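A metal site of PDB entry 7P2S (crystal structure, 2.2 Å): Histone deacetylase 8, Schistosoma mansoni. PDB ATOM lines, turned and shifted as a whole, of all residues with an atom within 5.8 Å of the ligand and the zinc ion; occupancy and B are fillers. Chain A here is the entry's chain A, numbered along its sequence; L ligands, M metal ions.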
ATOM      1  N   LYS A  20     -20.305 -29.351  26.706  1.00  0.00           N
ATOM      2  CA  LYS A  20     -19.648 -28.240  25.980  1.00  0.00           C
ATOM      3  C   LYS A  20     -19.463 -28.611  24.496  1.00  0.00           C
ATOM      4  O   LYS A  20     -19.801 -27.771  23.635  1.00  0.00           O
ATOM      5  CB  LYS A  20     -18.308 -27.901  26.640  1.00  0.00           C
ATOM      6  CG  LYS A  20     -17.455 -26.872  25.906  1.00  0.00           C
ATOM      7  CD  LYS A  20     -18.187 -25.573  25.620  1.00  0.00           C
ATOM      8  CE  LYS A  20     -17.373 -24.617  24.781  1.00  0.00           C
ATOM      9  NZ  LYS A  20     -15.981 -24.486  25.278  1.00  0.00           N
ATOM     10  N   TYR A  99     -15.973 -23.407  37.504  1.00  0.00           N
ATOM     11  CA  TYR A  99     -16.603 -22.412  36.588  1.00  0.00           C
ATOM     12  C   TYR A  99     -16.496 -22.902  35.137  1.00  0.00           C
ATOM     13  O   TYR A  99     -17.509 -23.410  34.614  1.00  0.00           O
ATOM     14  CB  TYR A  99     -15.985 -21.034  36.847  1.00  0.00           C
ATOM     15  CG  TYR A  99     -16.278 -20.494  38.224  1.00  0.00           C
ATOM     16  CD1 TYR A  99     -17.517 -19.944  38.524  1.00  0.00           C
ATOM     17  CD2 TYR A  99     -15.335 -20.537  39.237  1.00  0.00           C
ATOM     18  CE1 TYR A  99     -17.798 -19.448  39.792  1.00  0.00           C
ATOM     19  CE2 TYR A  99     -15.594 -20.052  40.504  1.00  0.00           C
ATOM     20  CZ  TYR A  99     -16.841 -19.498  40.786  1.00  0.00           C
ATOM     21  OH  TYR A  99     -17.099 -19.017  42.029  1.00  0.00           O
ATOM     22  N   ASP A 100     -15.323 -22.748  34.508  1.00  0.00           N
ATOM     23  CA  ASP A 100     -15.111 -23.071  33.071  1.00  0.00           C
ATOM     24  C   ASP A 100     -15.007 -24.593  32.887  1.00  0.00           C
ATOM     25  O   ASP A 100     -15.165 -25.054  31.739  1.00  0.00           O
ATOM     26  CB  ASP A 100     -13.889 -22.356  32.504  1.00  0.00           C
ATOM     27  CG  ASP A 100     -14.219 -21.137  31.660  1.00  0.00           C
ATOM     28  OD1 ASP A 100     -15.298 -20.545  31.881  1.00  0.00           O
ATOM     29  OD2 ASP A 100     -13.388 -20.785  30.784  1.00  0.00           O
ATOM     30  N   CYS A 101     -14.754 -25.332  33.972  1.00  0.00           N
ATOM     31  CA  CYS A 101     -14.598 -26.802  33.972  1.00  0.00           C
ATOM     32  C   CYS A 101     -15.597 -27.404  34.960  1.00  0.00           C
ATOM     33  O   CYS A 101     -15.211 -27.932  36.004  1.00  0.00           O
ATOM     34  CB  CYS A 101     -13.151 -27.159  34.304  1.00  0.00           C
ATOM     35  SG  CYS A 101     -11.981 -26.121  33.392  1.00  0.00           S
ATOM     36  N   PRO A 102     -16.909 -27.341  34.654  1.00  0.00           N
ATOM     37  CA  PRO A 102     -17.934 -27.858  35.565  1.00  0.00           C
ATOM     38  C   PRO A 102     -17.906 -29.387  35.615  1.00  0.00           C
ATOM     39  O   PRO A 102     -17.323 -30.006  34.744  1.00  0.00           O
ATOM     40  CB  PRO A 102     -19.244 -27.353  34.957  1.00  0.00           C
ATOM     41  CG  PRO A 102     -18.953 -27.234  33.480  1.00  0.00           C
ATOM     42  CD  PRO A 102     -17.487 -26.821  33.409  1.00  0.00           C
ATOM     43  N   HIS A 141      -4.959 -29.107  25.472  1.00  0.00           N
ATOM     44  CA  HIS A 141      -3.643 -28.485  25.774  1.00  0.00           C
ATOM     45  C   HIS A 141      -3.640 -27.648  27.065  1.00  0.00           C
ATOM     46  O   HIS A 141      -2.532 -27.310  27.508  1.00  0.00           O
ATOM     47  CB  HIS A 141      -3.163 -27.658  24.557  1.00  0.00           C
ATOM     48  CG  HIS A 141      -4.104 -26.582  24.103  1.00  0.00           C
ATOM     49  ND1 HIS A 141      -3.725 -25.645  23.153  1.00  0.00           N
ATOM     50  CD2 HIS A 141      -5.367 -26.271  24.445  1.00  0.00           C
ATOM     51  CE1 HIS A 141      -4.719 -24.815  22.933  1.00  0.00           C
ATOM     52  NE2 HIS A 141      -5.743 -25.182  23.707  1.00  0.00           N
ATOM     53  N   HIS A 142      -4.797 -27.348  27.662  1.00  0.00           N
ATOM     54  CA  HIS A 142      -4.913 -26.404  28.810  1.00  0.00           C
ATOM     55  C   HIS A 142      -4.745 -27.108  30.167  1.00  0.00           C
ATOM     56  O   HIS A 142      -4.341 -26.433  31.125  1.00  0.00           O
ATOM     57  CB  HIS A 142      -6.240 -25.635  28.771  1.00  0.00           C
ATOM     58  CG  HIS A 142      -6.325 -24.634  27.679  1.00  0.00           C
ATOM     59  ND1 HIS A 142      -5.287 -23.766  27.394  1.00  0.00           N
ATOM     60  CD2 HIS A 142      -7.303 -24.344  26.799  1.00  0.00           C
ATOM     61  CE1 HIS A 142      -5.630 -22.990  26.382  1.00  0.00           C
ATOM     62  NE2 HIS A 142      -6.864 -23.327  26.004  1.00  0.00           N
ATOM     63  N   GLY A 150     -10.129 -24.355  30.854  1.00  0.00           N
ATOM     64  CA  GLY A 150     -10.653 -24.197  29.480  1.00  0.00           C
ATOM     65  C   GLY A 150     -11.315 -25.459  28.947  1.00  0.00           C
ATOM     66  O   GLY A 150     -11.098 -25.785  27.755  1.00  0.00           O
ATOM     67  N   PHE A 151     -12.083 -26.141  29.801  1.00  0.00           N
ATOM     68  CA  PHE A 151     -12.784 -27.421  29.539  1.00  0.00           C
ATOM     69  C   PHE A 151     -11.781 -28.523  29.146  1.00  0.00           C
ATOM     70  O   PHE A 151     -12.177 -29.461  28.435  1.00  0.00           O
ATOM     71  CB  PHE A 151     -13.879 -27.275  28.486  1.00  0.00           C
ATOM     72  CG  PHE A 151     -14.987 -28.289  28.635  1.00  0.00           C
ATOM     73  CD1 PHE A 151     -15.959 -28.140  29.604  1.00  0.00           C
ATOM     74  CD2 PHE A 151     -15.036 -29.416  27.820  1.00  0.00           C
ATOM     75  CE1 PHE A 151     -16.969 -29.090  29.763  1.00  0.00           C
ATOM     76  CE2 PHE A 151     -16.049 -30.353  27.973  1.00  0.00           C
ATOM     77  CZ  PHE A 151     -17.011 -30.185  28.943  1.00  0.00           C
ATOM     78  N   CYS A 152     -10.542 -28.416  29.612  1.00  0.00           N
ATOM     79  CA  CYS A 152      -9.516 -29.498  29.565  1.00  0.00           C
ATOM     80  C   CYS A 152      -9.296 -29.996  30.994  1.00  0.00           C
ATOM     81  O   CYS A 152      -8.921 -29.167  31.851  1.00  0.00           O
ATOM     82  CB  CYS A 152      -8.220 -28.990  28.941  1.00  0.00           C
ATOM     83  SG  CYS A 152      -8.442 -28.249  27.302  1.00  0.00           S
ATOM     84  N   ASP A 186      -4.092 -24.091  17.486  1.00  0.00           N
ATOM     85  CA  ASP A 186      -5.329 -23.607  18.148  1.00  0.00           C
ATOM     86  C   ASP A 186      -5.285 -22.077  18.271  1.00  0.00           C
ATOM     87  O   ASP A 186      -4.168 -21.518  18.346  1.00  0.00           O
ATOM     88  CB  ASP A 186      -5.486 -24.250  19.539  1.00  0.00           C
ATOM     89  CG  ASP A 186      -6.866 -24.117  20.150  1.00  0.00           C
ATOM     90  OD1 ASP A 186      -7.180 -23.023  20.660  1.00  0.00           O
ATOM     91  OD2 ASP A 186      -7.589 -25.125  20.157  1.00  0.00           O
ATOM     92  N   LEU A 187      -6.450 -21.424  18.320  1.00  0.00           N
ATOM     93  CA  LEU A 187      -6.599 -19.965  18.517  1.00  0.00           C
ATOM     94  C   LEU A 187      -5.960 -19.538  19.853  1.00  0.00           C
ATOM     95  O   LEU A 187      -5.443 -18.403  19.916  1.00  0.00           O
ATOM     96  CB  LEU A 187      -8.081 -19.606  18.493  1.00  0.00           C
ATOM     97  CG  LEU A 187      -8.416 -18.133  18.717  1.00  0.00           C
ATOM     98  CD1 LEU A 187      -7.871 -17.280  17.581  1.00  0.00           C
ATOM     99  CD2 LEU A 187      -9.910 -17.927  18.880  1.00  0.00           C
ATOM    100  N   HIS A 188      -6.005 -20.416  20.857  1.00  0.00           N
ATOM    101  CA  HIS A 188      -5.556 -20.172  22.256  1.00  0.00           C
ATOM    102  C   HIS A 188      -4.132 -20.700  22.458  1.00  0.00           C
ATOM    103  O   HIS A 188      -3.779 -21.720  21.817  1.00  0.00           O
ATOM    104  CB  HIS A 188      -6.540 -20.807  23.250  1.00  0.00           C
ATOM    105  CG  HIS A 188      -7.916 -20.248  23.195  1.00  0.00           C
ATOM    106  ND1 HIS A 188      -8.933 -20.837  22.470  1.00  0.00           N
ATOM    107  CD2 HIS A 188      -8.442 -19.132  23.746  1.00  0.00           C
ATOM    108  CE1 HIS A 188     -10.038 -20.113  22.593  1.00  0.00           C
ATOM    109  NE2 HIS A 188      -9.750 -19.062  23.372  1.00  0.00           N
ATOM    110  N   PHE A 216      -8.171 -15.302  27.123  1.00  0.00           N
ATOM    111  CA  PHE A 216      -7.796 -16.616  27.695  1.00  0.00           C
ATOM    112  C   PHE A 216      -6.656 -17.232  26.889  1.00  0.00           C
ATOM    113  O   PHE A 216      -6.670 -17.172  25.661  1.00  0.00           O
ATOM    114  CB  PHE A 216      -9.016 -17.551  27.689  1.00  0.00           C
ATOM    115  CG  PHE A 216      -8.798 -18.841  28.437  1.00  0.00           C
ATOM    116  CD1 PHE A 216      -8.249 -19.938  27.813  1.00  0.00           C
ATOM    117  CD2 PHE A 216      -9.144 -18.943  29.785  1.00  0.00           C
ATOM    118  CE1 PHE A 216      -8.061 -21.128  28.502  1.00  0.00           C
ATOM    119  CE2 PHE A 216      -8.942 -20.125  30.481  1.00  0.00           C
ATOM    120  CZ  PHE A 216      -8.405 -21.215  29.830  1.00  0.00           C
ATOM    121  N   GLN A 281      -1.370 -30.063  17.538  1.00  0.00           N
ATOM    122  CA  GLN A 281      -2.729 -29.674  18.000  1.00  0.00           C
ATOM    123  C   GLN A 281      -3.353 -28.816  16.896  1.00  0.00           C
ATOM    124  O   GLN A 281      -2.749 -27.774  16.555  1.00  0.00           O
ATOM    125  CB  GLN A 281      -2.640 -28.962  19.352  1.00  0.00           C
ATOM    126  CG  GLN A 281      -3.926 -29.003  20.165  1.00  0.00           C
ATOM    127  CD  GLN A 281      -4.874 -27.876  19.831  1.00  0.00           C
ATOM    128  OE1 GLN A 281      -4.776 -27.231  18.793  1.00  0.00           O
ATOM    129  NE2 GLN A 281      -5.809 -27.622  20.748  1.00  0.00           N
ATOM    130  N   ASP A 285     -10.624 -23.308  16.009  1.00  0.00           N
ATOM    131  CA  ASP A 285     -11.246 -22.040  16.477  1.00  0.00           C
ATOM    132  C   ASP A 285     -10.551 -20.815  15.858  1.00  0.00           C
ATOM    133  O   ASP A 285     -10.932 -19.693  16.236  1.00  0.00           O
ATOM    134  CB  ASP A 285     -11.320 -21.968  18.007  1.00  0.00           C
ATOM    135  CG  ASP A 285     -10.110 -22.497  18.763  1.00  0.00           C
ATOM    136  OD1 ASP A 285      -9.067 -22.761  18.134  1.00  0.00           O
ATOM    137  OD2 ASP A 285     -10.242 -22.642  19.994  1.00  0.00           O
ATOM    138  N   ASP A 290     -15.842 -19.520  13.206  1.00  0.00           N
ATOM    139  CA  ASP A 290     -15.873 -19.863  14.653  1.00  0.00           C
ATOM    140  C   ASP A 290     -16.560 -18.716  15.395  1.00  0.00           C
ATOM    141  O   ASP A 290     -16.316 -17.553  15.065  1.00  0.00           O
ATOM    142  CB  ASP A 290     -14.483 -20.145  15.223  1.00  0.00           C
ATOM    143  CG  ASP A 290     -14.550 -20.797  16.595  1.00  0.00           C
ATOM    144  OD1 ASP A 290     -14.636 -22.039  16.642  1.00  0.00           O
ATOM    145  OD2 ASP A 290     -14.579 -20.056  17.589  1.00  0.00           O
ATOM    146  N   PRO A 291     -17.438 -19.002  16.378  1.00  0.00           N
ATOM    147  CA  PRO A 291     -18.122 -17.943  17.139  1.00  0.00           C
ATOM    148  C   PRO A 291     -17.190 -16.957  17.870  1.00  0.00           C
ATOM    149  O   PRO A 291     -17.640 -15.868  18.156  1.00  0.00           O
ATOM    150  CB  PRO A 291     -19.008 -18.711  18.143  1.00  0.00           C
ATOM    151  CG  PRO A 291     -18.471 -20.122  18.154  1.00  0.00           C
ATOM    152  CD  PRO A 291     -17.878 -20.350  16.784  1.00  0.00           C
ATOM    153  N   HIS A 292     -15.933 -17.336  18.131  1.00  0.00           N
ATOM    154  CA  HIS A 292     -14.876 -16.433  18.682  1.00  0.00           C
ATOM    155  C   HIS A 292     -14.704 -15.224  17.766  1.00  0.00           C
ATOM    156  O   HIS A 292     -14.559 -14.097  18.290  1.00  0.00           O
ATOM    157  CB  HIS A 292     -13.564 -17.207  18.895  1.00  0.00           C
ATOM    158  CG  HIS A 292     -13.504 -17.984  20.164  1.00  0.00           C
ATOM    159  ND1 HIS A 292     -13.818 -19.330  20.223  1.00  0.00           N
ATOM    160  CD2 HIS A 292     -13.165 -17.623  21.419  1.00  0.00           C
ATOM    161  CE1 HIS A 292     -13.682 -19.751  21.462  1.00  0.00           C
ATOM    162  NE2 HIS A 292     -13.282 -18.722  22.221  1.00  0.00           N
ATOM    163  N   GLY A 338      -8.938 -30.372  19.323  1.00  0.00           N
ATOM    164  CA  GLY A 338      -8.914 -29.349  20.377  1.00  0.00           C
ATOM    165  C   GLY A 338     -10.109 -28.421  20.260  1.00  0.00           C
ATOM    166  O   GLY A 338     -11.230 -28.931  20.077  1.00  0.00           O
ATOM    167  N   GLY A 339      -9.880 -27.106  20.331  1.00  0.00           N
ATOM    168  CA  GLY A 339     -10.900 -26.071  20.125  1.00  0.00           C
ATOM    169  C   GLY A 339     -11.581 -26.192  18.782  1.00  0.00           C
ATOM    170  O   GLY A 339     -11.057 -26.896  17.889  1.00  0.00           O
ATOM    171  N   GLY A 340     -12.732 -25.517  18.630  1.00  0.00           N
ATOM    172  CA  GLY A 340     -13.595 -25.554  17.435  1.00  0.00           C
ATOM    173  C   GLY A 340     -15.048 -25.649  17.865  1.00  0.00           C
ATOM    174  O   GLY A 340     -15.470 -26.752  18.244  1.00  0.00           O
ATOM    175  N   TYR A 341     -15.776 -24.540  17.825  1.00  0.00           N
ATOM    176  CA  TYR A 341     -17.116 -24.394  18.456  1.00  0.00           C
ATOM    177  C   TYR A 341     -18.215 -24.186  17.402  1.00  0.00           C
ATOM    178  O   TYR A 341     -19.397 -24.222  17.788  1.00  0.00           O
ATOM    179  CB  TYR A 341     -17.043 -23.307  19.531  1.00  0.00           C
ATOM    180  CG  TYR A 341     -15.910 -23.571  20.476  1.00  0.00           C
ATOM    181  CD1 TYR A 341     -16.041 -24.524  21.472  1.00  0.00           C
ATOM    182  CD2 TYR A 341     -14.678 -22.974  20.310  1.00  0.00           C
ATOM    183  CE1 TYR A 341     -14.981 -24.829  22.313  1.00  0.00           C
ATOM    184  CE2 TYR A 341     -13.612 -23.266  21.141  1.00  0.00           C
ATOM    185  CZ  TYR A 341     -13.770 -24.202  22.154  1.00  0.00           C
ATOM    186  OH  TYR A 341     -12.742 -24.505  22.998  1.00  0.00           O
HETATM  187  C1  LIG L   1     -17.325 -23.114  27.914  1.00  0.00           C
HETATM  188  C2  LIG L   1     -16.639 -23.760  28.907  1.00  0.00           C
HETATM  189  N1  LIG L   1     -14.804 -20.910  26.545  1.00  0.00           N
HETATM  190  C3  LIG L   1     -15.299 -23.516  29.190  1.00  0.00           C
HETATM  191  C4  LIG L   1     -14.617 -22.570  28.450  1.00  0.00           C
HETATM  192  C5  LIG L   1     -15.282 -21.898  27.433  1.00  0.00           C
HETATM  193  C6  LIG L   1     -16.654 -22.159  27.148  1.00  0.00           C
HETATM  194  C7  LIG L   1     -15.864 -20.592  25.731  1.00  0.00           C
HETATM  195  C8  LIG L   1     -16.984 -21.305  26.074  1.00  0.00           C
HETATM  196  C9  LIG L   1     -16.022 -19.622  24.616  1.00  0.00           C
HETATM  197  C10 LIG L   1     -17.216 -20.179  23.808  1.00  0.00           C
HETATM  198  C11 LIG L   1     -17.899 -19.111  22.982  1.00  0.00           C
HETATM  199  C12 LIG L   1     -17.145 -18.120  22.370  1.00  0.00           C
HETATM  200  C13 LIG L   1     -17.760 -17.118  21.620  1.00  0.00           C
HETATM  201  C14 LIG L   1     -19.126 -17.114  21.465  1.00  0.00           C
HETATM  202  C15 LIG L   1     -19.888 -18.100  22.059  1.00  0.00           C
HETATM  203  C16 LIG L   1     -19.272 -19.092  22.812  1.00  0.00           C
HETATM  204  N2  LIG L   1      -8.868 -23.685  24.002  1.00  0.00           N
HETATM  205  C17 LIG L   1     -13.468 -20.331  26.499  1.00  0.00           C
HETATM  206  C18 LIG L   1     -12.448 -21.368  26.208  1.00  0.00           C
HETATM  207  C19 LIG L   1     -10.854 -22.687  24.912  1.00  0.00           C
HETATM  208  C20 LIG L   1     -10.450 -22.510  26.221  1.00  0.00           C
HETATM  209  C21 LIG L   1     -11.418 -21.839  26.980  1.00  0.00           C
HETATM  210  C22 LIG L   1     -10.095 -23.253  23.766  1.00  0.00           C
HETATM  211  O1  LIG L   1     -10.612 -23.298  22.646  1.00  0.00           O
HETATM  212  S1  LIG L   1     -18.351 -20.913  25.052  1.00  0.00           S
HETATM  213  F1  LIG L   1     -17.294 -24.701  29.659  1.00  0.00           F
HETATM  214  S2  LIG L   1     -12.478 -22.158  24.672  1.00  0.00           S
HETATM  215  O2  LIG L   1      -8.006 -23.984  22.957  1.00  0.00           O
HETATM  216 ZN    ZN M   1      -8.928 -22.775  21.497  1.00  0.00          ZN
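N of Gly 339 sits at hydrogen-bond distance from OD2 of Asp 186. The side-chain amide nitrogen (NE2) of Gln 281 is in hydrogen-bond range of the side-chain carboxylate (OD2) of Asp 186. OD1 of Asp 285 is in hydrogen-bond range of N of Leu 187 (2.9 Å). NE2 of His 142 sits at hydrogen-bond distance from NE2 of His 141 (3.2 Å). The backbone NH of His 142 lies close to the side-chain sulfur of Cys 152 (3.8 Å). The backbone NH (N) of Gly 150 is in hydrogen-bond range of the side-chain sulfur (SG) of Cys 101, 3.6 Å away. N of Phe 151 is in hydrogen-bond range of SG of Cys 101 (3.6 Å). OD2 of Asp 290 is in hydrogen-bond range of ND1 of His 292 (2.8 Å).
The side-chain hydroxyl (OH) of Tyr 341 lies close to a sulfur (S2) of the ligand, at 2.9 Å. NE2 of His 141 lies within hydrogen-bond range of N2 of the ligand (3.5 Å). A ring nitrogen (NE2) of His 142 sits at hydrogen-bond distance from a nitrogen (N2) of the ligand.
O of Asp 100 sits close to F1 of the ligand. Residues that only touch the ligand: Lys 20 (3.1 Å), Gly 150 (3.5 Å), Phe 151 (3.7 Å), Phe 216 (3.6 Å), Pro 291 (3.7 Å), His 292 (3.7 Å) and Gly 339 (3.8 Å). Hydrophobic or aromatic side chains that line the ligand: His 141, His 142, Phe 151, His 188, Phe 216, Pro 291, His 292 and Tyr 341. Of the 23 residues printed, 14 come within 4 Å of the ligand.
The zinc ion is bound by OD1 of Asp 186 (2.0 Å), OD2 of Asp 285 (2.0 Å), O1 of the ligand (2.1 Å), O2 of the ligand (2.1 Å) and ND1 of His 188 (2.2 Å).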
